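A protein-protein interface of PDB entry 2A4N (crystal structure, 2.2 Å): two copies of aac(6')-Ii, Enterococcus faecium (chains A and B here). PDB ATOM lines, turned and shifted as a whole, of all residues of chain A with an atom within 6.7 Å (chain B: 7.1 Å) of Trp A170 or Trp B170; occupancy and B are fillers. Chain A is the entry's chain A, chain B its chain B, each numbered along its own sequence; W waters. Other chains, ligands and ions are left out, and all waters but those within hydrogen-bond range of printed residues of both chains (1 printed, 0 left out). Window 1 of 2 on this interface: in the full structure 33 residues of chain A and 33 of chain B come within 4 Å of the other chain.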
ATOM      1  N   TYR A  66      12.420 -23.189 -30.115  1.00  0.00           N
ATOM      2  CA  TYR A  66      12.538 -22.989 -31.556  1.00  0.00           C
ATOM      3  C   TYR A  66      13.931 -23.434 -31.966  1.00  0.00           C
ATOM      4  O   TYR A  66      14.895 -22.690 -31.791  1.00  0.00           O
ATOM      5  CB  TYR A  66      12.372 -21.515 -31.923  1.00  0.00           C
ATOM      6  CG  TYR A  66      11.080 -20.883 -31.464  1.00  0.00           C
ATOM      7  CD1 TYR A  66      10.932 -20.413 -30.162  1.00  0.00           C
ATOM      8  CD2 TYR A  66      10.009 -20.735 -32.341  1.00  0.00           C
ATOM      9  CE1 TYR A  66       9.749 -19.801 -29.749  1.00  0.00           C
ATOM     10  CE2 TYR A  66       8.819 -20.128 -31.936  1.00  0.00           C
ATOM     11  CZ  TYR A  66       8.700 -19.663 -30.644  1.00  0.00           C
ATOM     12  OH  TYR A  66       7.537 -19.049 -30.256  1.00  0.00           O
ATOM     13  N   GLU A  72      12.780 -20.506 -23.967  1.00  0.00           N
ATOM     14  CA  GLU A  72      11.857 -19.908 -23.023  1.00  0.00           C
ATOM     15  C   GLU A  72      12.483 -19.994 -21.637  1.00  0.00           C
ATOM     16  O   GLU A  72      12.878 -21.074 -21.194  1.00  0.00           O
ATOM     17  CB  GLU A  72      10.509 -20.639 -23.015  1.00  0.00           C
ATOM     18  CG  GLU A  72       9.695 -20.357 -21.754  1.00  0.00           C
ATOM     19  CD  GLU A  72       8.277 -20.898 -21.814  1.00  0.00           C
ATOM     20  OE1 GLU A  72       8.060 -21.987 -22.391  1.00  0.00           O
ATOM     21  OE2 GLU A  72       7.376 -20.234 -21.267  1.00  0.00           O
ATOM     22  N   TYR A 108      12.919 -15.762 -24.269  1.00  0.00           N
ATOM     23  CA  TYR A 108      11.658 -15.064 -24.016  1.00  0.00           C
ATOM     24  C   TYR A 108      10.977 -15.706 -22.818  1.00  0.00           C
ATOM     25  O   TYR A 108      11.391 -16.765 -22.361  1.00  0.00           O
ATOM     26  CB  TYR A 108      10.729 -15.130 -25.229  1.00  0.00           C
ATOM     27  CG  TYR A 108      10.088 -16.483 -25.439  1.00  0.00           C
ATOM     28  CD1 TYR A 108      10.796 -17.535 -26.017  1.00  0.00           C
ATOM     29  CD2 TYR A 108       8.771 -16.719 -25.034  1.00  0.00           C
ATOM     30  CE1 TYR A 108      10.210 -18.793 -26.190  1.00  0.00           C
ATOM     31  CE2 TYR A 108       8.176 -17.968 -25.202  1.00  0.00           C
ATOM     32  CZ  TYR A 108       8.903 -18.998 -25.782  1.00  0.00           C
ATOM     33  OH  TYR A 108       8.313 -20.225 -25.959  1.00  0.00           O
ATOM     34  N   LEU A 109       9.931 -15.060 -22.320  1.00  0.00           N
ATOM     35  CA  LEU A 109       9.202 -15.565 -21.170  1.00  0.00           C
ATOM     36  C   LEU A 109       7.815 -14.958 -21.124  1.00  0.00           C
ATOM     37  O   LEU A 109       7.524 -13.977 -21.808  1.00  0.00           O
ATOM     38  CB  LEU A 109       9.954 -15.216 -19.879  1.00  0.00           C
ATOM     39  CG  LEU A 109      10.295 -13.724 -19.722  1.00  0.00           C
ATOM     40  CD1 LEU A 109       9.165 -12.999 -19.001  1.00  0.00           C
ATOM     41  CD2 LEU A 109      11.594 -13.567 -18.944  1.00  0.00           C
ATOM     42  N   GLY A 110       6.966 -15.569 -20.310  1.00  0.00           N
ATOM     43  CA  GLY A 110       5.615 -15.092 -20.127  1.00  0.00           C
ATOM     44  C   GLY A 110       5.419 -14.836 -18.645  1.00  0.00           C
ATOM     45  O   GLY A 110       5.445 -15.771 -17.837  1.00  0.00           O
ATOM     46  N   THR A 111       5.262 -13.571 -18.274  1.00  0.00           N
ATOM     47  CA  THR A 111       5.037 -13.227 -16.873  1.00  0.00           C
ATOM     48  C   THR A 111       3.566 -12.841 -16.750  1.00  0.00           C
ATOM     49  O   THR A 111       3.112 -11.868 -17.352  1.00  0.00           O
ATOM     50  CB  THR A 111       5.958 -12.060 -16.403  1.00  0.00           C
ATOM     51  OG1 THR A 111       5.661 -11.738 -15.039  1.00  0.00           O
ATOM     52  CG2 THR A 111       5.769 -10.824 -17.271  1.00  0.00           C
ATOM     53  N   VAL A 133       0.644  -1.502 -24.183  1.00  0.00           N
ATOM     54  CA  VAL A 133       1.892  -2.200 -23.880  1.00  0.00           C
ATOM     55  C   VAL A 133       3.008  -1.175 -23.658  1.00  0.00           C
ATOM     56  O   VAL A 133       3.698  -1.197 -22.641  1.00  0.00           O
ATOM     57  CB  VAL A 133       2.312  -3.143 -25.047  1.00  0.00           C
ATOM     58  CG1 VAL A 133       3.734  -3.640 -24.837  1.00  0.00           C
ATOM     59  CG2 VAL A 133       1.354  -4.324 -25.138  1.00  0.00           C
ATOM     60  N   LYS A 153      12.337  -6.921 -23.121  1.00  0.00           N
ATOM     61  CA  LYS A 153      11.320  -5.990 -23.580  1.00  0.00           C
ATOM     62  C   LYS A 153       9.965  -6.667 -23.775  1.00  0.00           C
ATOM     63  O   LYS A 153       9.886  -7.804 -24.246  1.00  0.00           O
ATOM     64  CB  LYS A 153      11.780  -5.363 -24.912  1.00  0.00           C
ATOM     65  CG  LYS A 153      10.731  -4.547 -25.642  1.00  0.00           C
ATOM     66  CD  LYS A 153      11.229  -4.111 -27.014  1.00  0.00           C
ATOM     67  CE  LYS A 153      10.342  -3.027 -27.605  1.00  0.00           C
ATOM     68  NZ  LYS A 153      10.844  -2.555 -28.915  1.00  0.00           N
ATOM     69  N   ILE A 154       8.896  -5.965 -23.420  1.00  0.00           N
ATOM     70  CA  ILE A 154       7.564  -6.522 -23.610  1.00  0.00           C
ATOM     71  C   ILE A 154       7.331  -6.524 -25.114  1.00  0.00           C
ATOM     72  O   ILE A 154       7.374  -5.475 -25.758  1.00  0.00           O
ATOM     73  CB  ILE A 154       6.471  -5.674 -22.921  1.00  0.00           C
ATOM     74  CG1 ILE A 154       6.698  -5.657 -21.411  1.00  0.00           C
ATOM     75  CG2 ILE A 154       5.095  -6.279 -23.183  1.00  0.00           C
ATOM     76  CD1 ILE A 154       5.689  -4.813 -20.648  1.00  0.00           C
ATOM     77  N   VAL A 155       7.099  -7.702 -25.676  1.00  0.00           N
ATOM     78  CA  VAL A 155       6.884  -7.806 -27.111  1.00  0.00           C
ATOM     79  C   VAL A 155       5.495  -8.326 -27.473  1.00  0.00           C
ATOM     80  O   VAL A 155       5.177  -8.521 -28.645  1.00  0.00           O
ATOM     81  CB  VAL A 155       7.966  -8.697 -27.753  1.00  0.00           C
ATOM     82  CG1 VAL A 155       9.298  -7.956 -27.768  1.00  0.00           C
ATOM     83  CG2 VAL A 155       8.101  -9.997 -26.974  1.00  0.00           C
ATOM     84  N   GLY A 156       4.662  -8.545 -26.466  1.00  0.00           N
ATOM     85  CA  GLY A 156       3.320  -9.020 -26.730  1.00  0.00           C
ATOM     86  C   GLY A 156       2.518  -9.270 -25.470  1.00  0.00           C
ATOM     87  O   GLY A 156       3.049  -9.229 -24.356  1.00  0.00           O
ATOM     88  N   VAL A 157       1.225  -9.510 -25.655  1.00  0.00           N
ATOM     89  CA  VAL A 157       0.318  -9.803 -24.557  1.00  0.00           C
ATOM     90  C   VAL A 157      -0.711 -10.838 -25.003  1.00  0.00           C
ATOM     91  O   VAL A 157      -1.076 -10.912 -26.182  1.00  0.00           O
ATOM     92  CB  VAL A 157      -0.441  -8.541 -24.057  1.00  0.00           C
ATOM     93  CG1 VAL A 157       0.513  -7.603 -23.330  1.00  0.00           C
ATOM     94  CG2 VAL A 157      -1.107  -7.831 -25.228  1.00  0.00           C
ATOM     95  N   LEU A 158      -1.168 -11.641 -24.050  1.00  0.00           N
ATOM     96  CA  LEU A 158      -2.172 -12.657 -24.316  1.00  0.00           C
ATOM     97  C   LEU A 158      -3.414 -12.251 -23.530  1.00  0.00           C
ATOM     98  O   LEU A 158      -3.535 -12.528 -22.339  1.00  0.00           O
ATOM     99  CB  LEU A 158      -1.664 -14.038 -23.873  1.00  0.00           C
ATOM    100  CG  LEU A 158      -2.560 -15.251 -24.157  1.00  0.00           C
ATOM    101  CD1 LEU A 158      -3.172 -15.134 -25.544  1.00  0.00           C
ATOM    102  CD2 LEU A 158      -1.742 -16.539 -24.033  1.00  0.00           C
ATOM    103  N   PRO A 159      -4.344 -11.553 -24.190  1.00  0.00           N
ATOM    104  CA  PRO A 159      -5.578 -11.103 -23.542  1.00  0.00           C
ATOM    105  C   PRO A 159      -6.365 -12.230 -22.880  1.00  0.00           C
ATOM    106  O   PRO A 159      -6.614 -13.270 -23.490  1.00  0.00           O
ATOM    107  CB  PRO A 159      -6.354 -10.465 -24.690  1.00  0.00           C
ATOM    108  CG  PRO A 159      -5.273  -9.950 -25.582  1.00  0.00           C
ATOM    109  CD  PRO A 159      -4.293 -11.097 -25.591  1.00  0.00           C
ATOM    110  N   ASP A 168      -1.188 -12.755 -19.898  1.00  0.00           N
ATOM    111  CA  ASP A 168       0.178 -13.206 -19.721  1.00  0.00           C
ATOM    112  C   ASP A 168       0.929 -12.108 -20.451  1.00  0.00           C
ATOM    113  O   ASP A 168       0.412 -11.537 -21.412  1.00  0.00           O
ATOM    114  CB  ASP A 168       0.427 -14.566 -20.392  1.00  0.00           C
ATOM    115  CG  ASP A 168       1.818 -15.122 -20.087  1.00  0.00           C
ATOM    116  OD1 ASP A 168       2.503 -14.577 -19.193  1.00  0.00           O
ATOM    117  OD2 ASP A 168       2.229 -16.110 -20.730  1.00  0.00           O
ATOM    118  N   ILE A 169       2.128 -11.780 -19.990  1.00  0.00           N
ATOM    119  CA  ILE A 169       2.901 -10.728 -20.638  1.00  0.00           C
ATOM    120  C   ILE A 169       4.172 -11.322 -21.226  1.00  0.00           C
ATOM    121  O   ILE A 169       5.017 -11.835 -20.492  1.00  0.00           O
ATOM    122  CB  ILE A 169       3.260  -9.612 -19.631  1.00  0.00           C
ATOM    123  CG1 ILE A 169       1.974  -9.035 -19.024  1.00  0.00           C
ATOM    124  CG2 ILE A 169       4.058  -8.507 -20.328  1.00  0.00           C
ATOM    125  CD1 ILE A 169       2.200  -8.135 -17.804  1.00  0.00           C
ATOM    126  N   TRP A 170       4.296 -11.260 -22.550  1.00  0.00           N
ATOM    127  CA  TRP A 170       5.472 -11.797 -23.226  1.00  0.00           C
ATOM    128  C   TRP A 170       6.599 -10.784 -23.296  1.00  0.00           C
ATOM    129  O   TRP A 170       6.401  -9.641 -23.702  1.00  0.00           O
ATOM    130  CB  TRP A 170       5.134 -12.267 -24.645  1.00  0.00           C
ATOM    131  CG  TRP A 170       4.419 -13.587 -24.703  1.00  0.00           C
ATOM    132  CD1 TRP A 170       4.844 -14.778 -24.172  1.00  0.00           C
ATOM    133  CD2 TRP A 170       3.171 -13.862 -25.355  1.00  0.00           C
ATOM    134  NE1 TRP A 170       3.934 -15.773 -24.455  1.00  0.00           N
ATOM    135  CE2 TRP A 170       2.899 -15.239 -25.179  1.00  0.00           C
ATOM    136  CE3 TRP A 170       2.255 -13.079 -26.072  1.00  0.00           C
ATOM    137  CZ2 TRP A 170       1.745 -15.852 -25.694  1.00  0.00           C
ATOM    138  CZ3 TRP A 170       1.105 -13.690 -26.586  1.00  0.00           C
ATOM    139  CH2 TRP A 170       0.864 -15.065 -26.392  1.00  0.00           C
ATOM    140  N   MET A 171       7.785 -11.222 -22.893  1.00  0.00           N
ATOM    141  CA  MET A 171       8.974 -10.384 -22.913  1.00  0.00           C
ATOM    142  C   MET A 171      10.092 -11.169 -23.581  1.00  0.00           C
ATOM    143  O   MET A 171      10.158 -12.388 -23.451  1.00  0.00           O
ATOM    144  CB  MET A 171       9.379 -10.015 -21.487  1.00  0.00           C
ATOM    145  CG  MET A 171       8.286  -9.300 -20.717  1.00  0.00           C
ATOM    146  SD  MET A 171       8.896  -8.620 -19.183  1.00  0.00           S
ATOM    147  CE  MET A 171       9.954  -7.240 -19.829  1.00  0.00           C
ATOM    148  N   ALA A 172      10.971 -10.479 -24.295  1.00  0.00           N
ATOM    149  CA  ALA A 172      12.066 -11.163 -24.966  1.00  0.00           C
ATOM    150  C   ALA A 172      13.345 -10.337 -25.039  1.00  0.00           C
ATOM    151  O   ALA A 172      13.342  -9.110 -24.866  1.00  0.00           O
ATOM    152  CB  ALA A 172      11.640 -11.568 -26.360  1.00  0.00           C
ATOM    153  N   TYR B  66      -3.070 -22.199 -19.989  1.00  0.00           N
ATOM    154  CA  TYR B  66      -3.318 -21.403 -18.787  1.00  0.00           C
ATOM    155  C   TYR B  66      -4.577 -21.975 -18.162  1.00  0.00           C
ATOM    156  O   TYR B  66      -5.687 -21.669 -18.602  1.00  0.00           O
ATOM    157  CB  TYR B  66      -3.519 -19.926 -19.153  1.00  0.00           C
ATOM    158  CG  TYR B  66      -2.338 -19.333 -19.895  1.00  0.00           C
ATOM    159  CD1 TYR B  66      -2.185 -19.526 -21.269  1.00  0.00           C
ATOM    160  CD2 TYR B  66      -1.345 -18.628 -19.212  1.00  0.00           C
ATOM    161  CE1 TYR B  66      -1.075 -19.033 -21.948  1.00  0.00           C
ATOM    162  CE2 TYR B  66      -0.231 -18.130 -19.877  1.00  0.00           C
ATOM    163  CZ  TYR B  66      -0.104 -18.337 -21.247  1.00  0.00           C
ATOM    164  OH  TYR B  66       0.990 -17.845 -21.917  1.00  0.00           O
ATOM    165  N   GLU B  72      -3.747 -22.972 -26.521  1.00  0.00           N
ATOM    166  CA  GLU B  72      -2.904 -22.704 -27.677  1.00  0.00           C
ATOM    167  C   GLU B  72      -3.388 -23.544 -28.858  1.00  0.00           C
ATOM    168  O   GLU B  72      -3.510 -24.770 -28.755  1.00  0.00           O
ATOM    169  CB  GLU B  72      -1.431 -23.053 -27.413  1.00  0.00           C
ATOM    170  CG  GLU B  72      -0.545 -22.679 -28.603  1.00  0.00           C
ATOM    171  CD  GLU B  72       0.839 -23.307 -28.577  1.00  0.00           C
ATOM    172  OE1 GLU B  72       1.293 -23.745 -27.496  1.00  0.00           O
ATOM    173  OE2 GLU B  72       1.476 -23.351 -29.655  1.00  0.00           O
ATOM    174  N   TYR B 108      -4.930 -18.801 -28.474  1.00  0.00           N
ATOM    175  CA  TYR B 108      -3.818 -18.085 -29.080  1.00  0.00           C
ATOM    176  C   TYR B 108      -2.981 -19.050 -29.905  1.00  0.00           C
ATOM    177  O   TYR B 108      -3.176 -20.267 -29.853  1.00  0.00           O
ATOM    178  CB  TYR B 108      -2.950 -17.390 -28.017  1.00  0.00           C
ATOM    179  CG  TYR B 108      -2.047 -18.316 -27.221  1.00  0.00           C
ATOM    180  CD1 TYR B 108      -2.560 -19.141 -26.220  1.00  0.00           C
ATOM    181  CD2 TYR B 108      -0.680 -18.372 -27.483  1.00  0.00           C
ATOM    182  CE1 TYR B 108      -1.731 -20.003 -25.500  1.00  0.00           C
ATOM    183  CE2 TYR B 108       0.155 -19.225 -26.770  1.00  0.00           C
ATOM    184  CZ  TYR B 108      -0.376 -20.039 -25.783  1.00  0.00           C
ATOM    185  OH  TYR B 108       0.451 -20.894 -25.094  1.00  0.00           O
ATOM    186  N   LEU B 109      -2.050 -18.501 -30.670  1.00  0.00           N
ATOM    187  CA  LEU B 109      -1.199 -19.313 -31.517  1.00  0.00           C
ATOM    188  C   LEU B 109       0.066 -18.566 -31.900  1.00  0.00           C
ATOM    189  O   LEU B 109       0.147 -17.343 -31.778  1.00  0.00           O
ATOM    190  CB  LEU B 109      -1.962 -19.708 -32.784  1.00  0.00           C
ATOM    191  CG  LEU B 109      -2.547 -18.541 -33.595  1.00  0.00           C
ATOM    192  CD1 LEU B 109      -1.456 -17.928 -34.482  1.00  0.00           C
ATOM    193  CD2 LEU B 109      -3.697 -19.045 -34.464  1.00  0.00           C
ATOM    194  N   GLY B 110       1.049 -19.328 -32.360  1.00  0.00           N
ATOM    195  CA  GLY B 110       2.304 -18.760 -32.799  1.00  0.00           C
ATOM    196  C   GLY B 110       2.499 -19.245 -34.223  1.00  0.00           C
ATOM    197  O   GLY B 110       2.653 -20.447 -34.452  1.00  0.00           O
ATOM    198  N   THR B 111       2.455 -18.325 -35.182  1.00  0.00           N
ATOM    199  CA  THR B 111       2.635 -18.687 -36.582  1.00  0.00           C
ATOM    200  C   THR B 111       3.963 -18.102 -37.051  1.00  0.00           C
ATOM    201  O   THR B 111       4.074 -16.904 -37.297  1.00  0.00           O
ATOM    202  CB  THR B 111       1.450 -18.163 -37.455  1.00  0.00           C
ATOM    203  OG1 THR B 111       1.697 -18.470 -38.831  1.00  0.00           O
ATOM    204  CG2 THR B 111       1.261 -16.657 -37.291  1.00  0.00           C
ATOM    205  N   VAL B 133       4.638  -4.170 -36.720  1.00  0.00           N
ATOM    206  CA  VAL B 133       3.531  -5.101 -36.558  1.00  0.00           C
ATOM    207  C   VAL B 133       2.263  -4.490 -37.147  1.00  0.00           C
ATOM    208  O   VAL B 133       1.504  -5.172 -37.819  1.00  0.00           O
ATOM    209  CB  VAL B 133       3.265  -5.432 -35.072  1.00  0.00           C
ATOM    210  CG1 VAL B 133       1.983  -6.263 -34.944  1.00  0.00           C
ATOM    211  CG2 VAL B 133       4.439  -6.192 -34.492  1.00  0.00           C
ATOM    212  N   LYS B 153      -6.252 -11.647 -33.840  1.00  0.00           N
ATOM    213  CA  LYS B 153      -5.462 -10.434 -33.996  1.00  0.00           C
ATOM    214  C   LYS B 153      -4.016 -10.636 -33.543  1.00  0.00           C
ATOM    215  O   LYS B 153      -3.751 -11.367 -32.589  1.00  0.00           O
ATOM    216  CB  LYS B 153      -6.088  -9.292 -33.191  1.00  0.00           C
ATOM    217  CG  LYS B 153      -5.291  -8.003 -33.252  1.00  0.00           C
ATOM    218  CD  LYS B 153      -5.832  -6.947 -32.306  1.00  0.00           C
ATOM    219  CE  LYS B 153      -4.988  -5.683 -32.390  1.00  0.00           C
ATOM    220  NZ  LYS B 153      -5.462  -4.642 -31.447  1.00  0.00           N
ATOM    221  N   ILE B 154      -3.084  -9.984 -34.228  1.00  0.00           N
ATOM    222  CA  ILE B 154      -1.679 -10.091 -33.860  1.00  0.00           C
ATOM    223  C   ILE B 154      -1.512  -9.276 -32.588  1.00  0.00           C
ATOM    224  O   ILE B 154      -1.755  -8.066 -32.580  1.00  0.00           O
ATOM    225  CB  ILE B 154      -0.751  -9.517 -34.950  1.00  0.00           C
ATOM    226  CG1 ILE B 154      -0.981 -10.259 -36.274  1.00  0.00           C
ATOM    227  CG2 ILE B 154       0.704  -9.631 -34.497  1.00  0.00           C
ATOM    228  CD1 ILE B 154      -0.195  -9.698 -37.458  1.00  0.00           C
ATOM    229  N   VAL B 155      -1.115  -9.955 -31.514  1.00  0.00           N
ATOM    230  CA  VAL B 155      -0.934  -9.325 -30.211  1.00  0.00           C
ATOM    231  C   VAL B 155       0.506  -9.425 -29.712  1.00  0.00           C
ATOM    232  O   VAL B 155       0.793  -9.104 -28.562  1.00  0.00           O
ATOM    233  CB  VAL B 155      -1.845  -9.986 -29.158  1.00  0.00           C
ATOM    234  CG1 VAL B 155      -3.304  -9.649 -29.432  1.00  0.00           C
ATOM    235  CG2 VAL B 155      -1.637 -11.494 -29.183  1.00  0.00           C
ATOM    236  N   GLY B 156       1.404  -9.888 -30.573  1.00  0.00           N
ATOM    237  CA  GLY B 156       2.795 -10.009 -30.177  1.00  0.00           C
ATOM    238  C   GLY B 156       3.671 -10.665 -31.223  1.00  0.00           C
ATOM    239  O   GLY B 156       3.185 -11.293 -32.166  1.00  0.00           O
ATOM    240  N   VAL B 157       4.977 -10.498 -31.056  1.00  0.00           N
ATOM    241  CA  VAL B 157       5.955 -11.083 -31.955  1.00  0.00           C
ATOM    242  C   VAL B 157       7.192 -11.420 -31.142  1.00  0.00           C
ATOM    243  O   VAL B 157       7.537 -10.698 -30.200  1.00  0.00           O
ATOM    244  CB  VAL B 157       6.370 -10.108 -33.100  1.00  0.00           C
ATOM    245  CG1 VAL B 157       5.183  -9.833 -34.010  1.00  0.00           C
ATOM    246  CG2 VAL B 157       6.920  -8.795 -32.514  1.00  0.00           C
ATOM    247  N   LEU B 158       7.841 -12.526 -31.492  1.00  0.00           N
ATOM    248  CA  LEU B 158       9.066 -12.939 -30.821  1.00  0.00           C
ATOM    249  C   LEU B 158      10.186 -12.729 -31.824  1.00  0.00           C
ATOM    250  O   LEU B 158      10.388 -13.541 -32.729  1.00  0.00           O
ATOM    251  CB  LEU B 158       9.017 -14.413 -30.421  1.00  0.00           C
ATOM    252  CG  LEU B 158      10.310 -14.943 -29.784  1.00  0.00           C
ATOM    253  CD1 LEU B 158      10.788 -13.991 -28.691  1.00  0.00           C
ATOM    254  CD2 LEU B 158      10.062 -16.332 -29.216  1.00  0.00           C
ATOM    255  N   PRO B 159      10.923 -11.623 -31.686  1.00  0.00           N
ATOM    256  CA  PRO B 159      12.018 -11.345 -32.614  1.00  0.00           C
ATOM    257  C   PRO B 159      13.088 -12.438 -32.629  1.00  0.00           C
ATOM    258  O   PRO B 159      13.452 -12.980 -31.584  1.00  0.00           O
ATOM    259  CB  PRO B 159      12.578 -10.016 -32.102  1.00  0.00           C
ATOM    260  CG  PRO B 159      11.403  -9.360 -31.465  1.00  0.00           C
ATOM    261  CD  PRO B 159      10.732 -10.510 -30.742  1.00  0.00           C
ATOM    262  N   ASP B 168       8.348 -15.260 -34.664  1.00  0.00           N
ATOM    263  CA  ASP B 168       7.133 -16.028 -34.466  1.00  0.00           C
ATOM    264  C   ASP B 168       6.120 -14.900 -34.308  1.00  0.00           C
ATOM    265  O   ASP B 168       6.438 -13.852 -33.736  1.00  0.00           O
ATOM    266  CB  ASP B 168       7.189 -16.871 -33.188  1.00  0.00           C
ATOM    267  CG  ASP B 168       6.079 -17.916 -33.132  1.00  0.00           C
ATOM    268  OD1 ASP B 168       5.304 -18.028 -34.104  1.00  0.00           O
ATOM    269  OD2 ASP B 168       5.982 -18.636 -32.121  1.00  0.00           O
ATOM    270  N   ILE B 169       4.922 -15.087 -34.840  1.00  0.00           N
ATOM    271  CA  ILE B 169       3.895 -14.059 -34.744  1.00  0.00           C
ATOM    272  C   ILE B 169       2.779 -14.583 -33.857  1.00  0.00           C
ATOM    273  O   ILE B 169       2.142 -15.588 -34.185  1.00  0.00           O
ATOM    274  CB  ILE B 169       3.317 -13.720 -36.134  1.00  0.00           C
ATOM    275  CG1 ILE B 169       4.449 -13.320 -37.083  1.00  0.00           C
ATOM    276  CG2 ILE B 169       2.309 -12.583 -36.017  1.00  0.00           C
ATOM    277  CD1 ILE B 169       3.991 -13.066 -38.513  1.00  0.00           C
ATOM    278  N   TRP B 170       2.555 -13.916 -32.729  1.00  0.00           N
ATOM    279  CA  TRP B 170       1.514 -14.335 -31.797  1.00  0.00           C
ATOM    280  C   TRP B 170       0.179 -13.691 -32.144  1.00  0.00           C
ATOM    281  O   TRP B 170       0.094 -12.479 -32.352  1.00  0.00           O
ATOM    282  CB  TRP B 170       1.894 -13.972 -30.359  1.00  0.00           C
ATOM    283  CG  TRP B 170       2.821 -14.945 -29.702  1.00  0.00           C
ATOM    284  CD1 TRP B 170       2.639 -16.295 -29.579  1.00  0.00           C
ATOM    285  CD2 TRP B 170       4.060 -14.644 -29.041  1.00  0.00           C
ATOM    286  NE1 TRP B 170       3.686 -16.852 -28.882  1.00  0.00           N
ATOM    287  CE2 TRP B 170       4.572 -15.863 -28.540  1.00  0.00           C
ATOM    288  CE3 TRP B 170       4.785 -13.467 -28.822  1.00  0.00           C
ATOM    289  CZ2 TRP B 170       5.780 -15.939 -27.833  1.00  0.00           C
ATOM    290  CZ3 TRP B 170       5.988 -13.541 -28.116  1.00  0.00           C
ATOM    291  CH2 TRP B 170       6.470 -14.771 -27.631  1.00  0.00           C
ATOM    292  N   MET B 171      -0.859 -14.513 -32.209  1.00  0.00           N
ATOM    293  CA  MET B 171      -2.199 -14.036 -32.525  1.00  0.00           C
ATOM    294  C   MET B 171      -3.165 -14.584 -31.485  1.00  0.00           C
ATOM    295  O   MET B 171      -2.939 -15.659 -30.929  1.00  0.00           O
ATOM    296  CB  MET B 171      -2.597 -14.500 -33.925  1.00  0.00           C
ATOM    297  CG  MET B 171      -1.691 -13.954 -35.007  1.00  0.00           C
ATOM    298  SD  MET B 171      -2.211 -14.381 -36.672  1.00  0.00           S
ATOM    299  CE  MET B 171      -3.709 -13.348 -36.804  1.00  0.00           C
ATOM    300  N   ALA B 172      -4.239 -13.847 -31.213  1.00  0.00           N
ATOM    301  CA  ALA B 172      -5.205 -14.297 -30.222  1.00  0.00           C
ATOM    302  C   ALA B 172      -6.619 -13.839 -30.522  1.00  0.00           C
ATOM    303  O   ALA B 172      -6.839 -12.877 -31.264  1.00  0.00           O
ATOM    304  CB  ALA B 172      -4.794 -13.817 -28.835  1.00  0.00           C
HETATM  305  O   HOH W   1       3.908 -18.457 -23.581  1.00  0.00           O
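The backbone NH of Val A155 lies within hydrogen-bond range of the backbone carbonyl oxygen of Trp A170 (2.9 Å).
O of Gly A156 is in hydrogen-bond range of N of Trp A170 (3.0 Å).
N of Leu B158 is in hydrogen-bond range of O of Asp B168 (3.0 Å).
The backbone carbonyl oxygen of Lys A153 is in hydrogen-bond range of the backbone NH of Ala A172 (2.9 Å).
The backbone carbonyl oxygen (O) of Trp B170 sits at hydrogen-bond distance from the backbone NH (N) of Val B155, at 2.9 Å.
N of Ala B172 is in hydrogen-bond range of O of Lys B153, at 2.9 Å.
Printed residues of chain B within 4 Å of Tyr A66: Leu B158 (3.5 Å) and Asp B168 (2.5 Å).
Ile A154 touches none of the printed residues of chain B.
Of the printed residues of chain B, Val A157 touches Val B155.
Trp A170 touches just these residues of chain B: Tyr B108 and Trp B170.
Of the printed residues of chain A, Tyr B66 touches Leu A158 and Asp A168.
Ile B154 touches none of the printed residues of chain A.
Of chain A, only Tyr A108 and Trp A170 come within 4 Å of Trp B170.
Of the printed residues of chain A, Ala B172 touches Leu A158.
The nearest residue of chain B that does not touch Trp A170 is Tyr B66 (4.3 Å).
O of Val B155 is in hydrogen-bond range of N of Val A157, at 3.0 Å.
The side-chain carboxylate of Asp B168 is in hydrogen-bond range of the side-chain hydroxyl of Tyr A66 (2.5 Å).
The side-chain carboxylate of Asp A168 lies within hydrogen-bond range of the side-chain hydroxyl of Tyr B66, 2.4 Å away.
The backbone carbonyl oxygen (O) of Val A155 lies within hydrogen-bond range of the backbone NH (N) of Val B157 (3.1 Å).
Of the 19 printed residues of chain A, 9 touch a printed residue of chain B.
Of the 19 printed residues of chain B, 9 touch a printed residue of chain A.
Printed residues of chain B that touch a printed residue of chain A: Tyr B66, Tyr B108, Val B155, Gly B156, Val B157, Leu B158, Asp B168, Trp B170 and Ala B172.
Hydrophobic or aromatic side chains of chain B that line the printed part of chain A: Tyr B66, Tyr B108, Val B155, Leu B158, Trp B170 and Ala B172.
Among the printed residues, 16 pairs touch across the chains.
Among the printed residues, no Asp or Glu carboxylate lies within 4 Å of a Lys or Arg side-chain nitrogen of the other chain.
Among the printed residues, pairs that only touch across the chains: Gly A156 with Val B155 (3.1 Å), Val A155 with Gly B156 (3.2 Å), Leu A158 with Tyr B66 (3.3 Å), Leu A158 with Tyr B108 (3.4 Å), Ala A172 with Leu B158 (3.5 Å), Tyr A108 with Leu B158 (3.5 Å), Tyr A66 with Leu B158 (3.5 Å), Gly A156 with Gly B156 (3.6 Å), Trp A170 with Trp B170 (3.8 Å), Trp A170 with Tyr B108 (3.8 Å), Leu A158 with Ala B172 (3.9 Å) and Tyr A108 with Trp B170 (3.98 Å).
Water W1 lies within hydrogen-bond range of NE1 of Trp A170 (2.8 Å) and OH of Tyr B66 (3.4 Å).
Tyr A108 touches Trp B170, and with the chains exchanged Trp A170 touches Tyr B108.
Gly B156 touches its own counterpart, Gly A156.
Leu A158 touches Ala B172, and with the chains exchanged Ala A172 touches Leu B158.
Trp A170 touches its own counterpart, Trp B170.
Positions printed for both chains: 66, 72, 108, 109, 110, 111, 133, 153, 154, 155, 156, 157, 158, 159, 168, 169, 170, 171 and 172.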
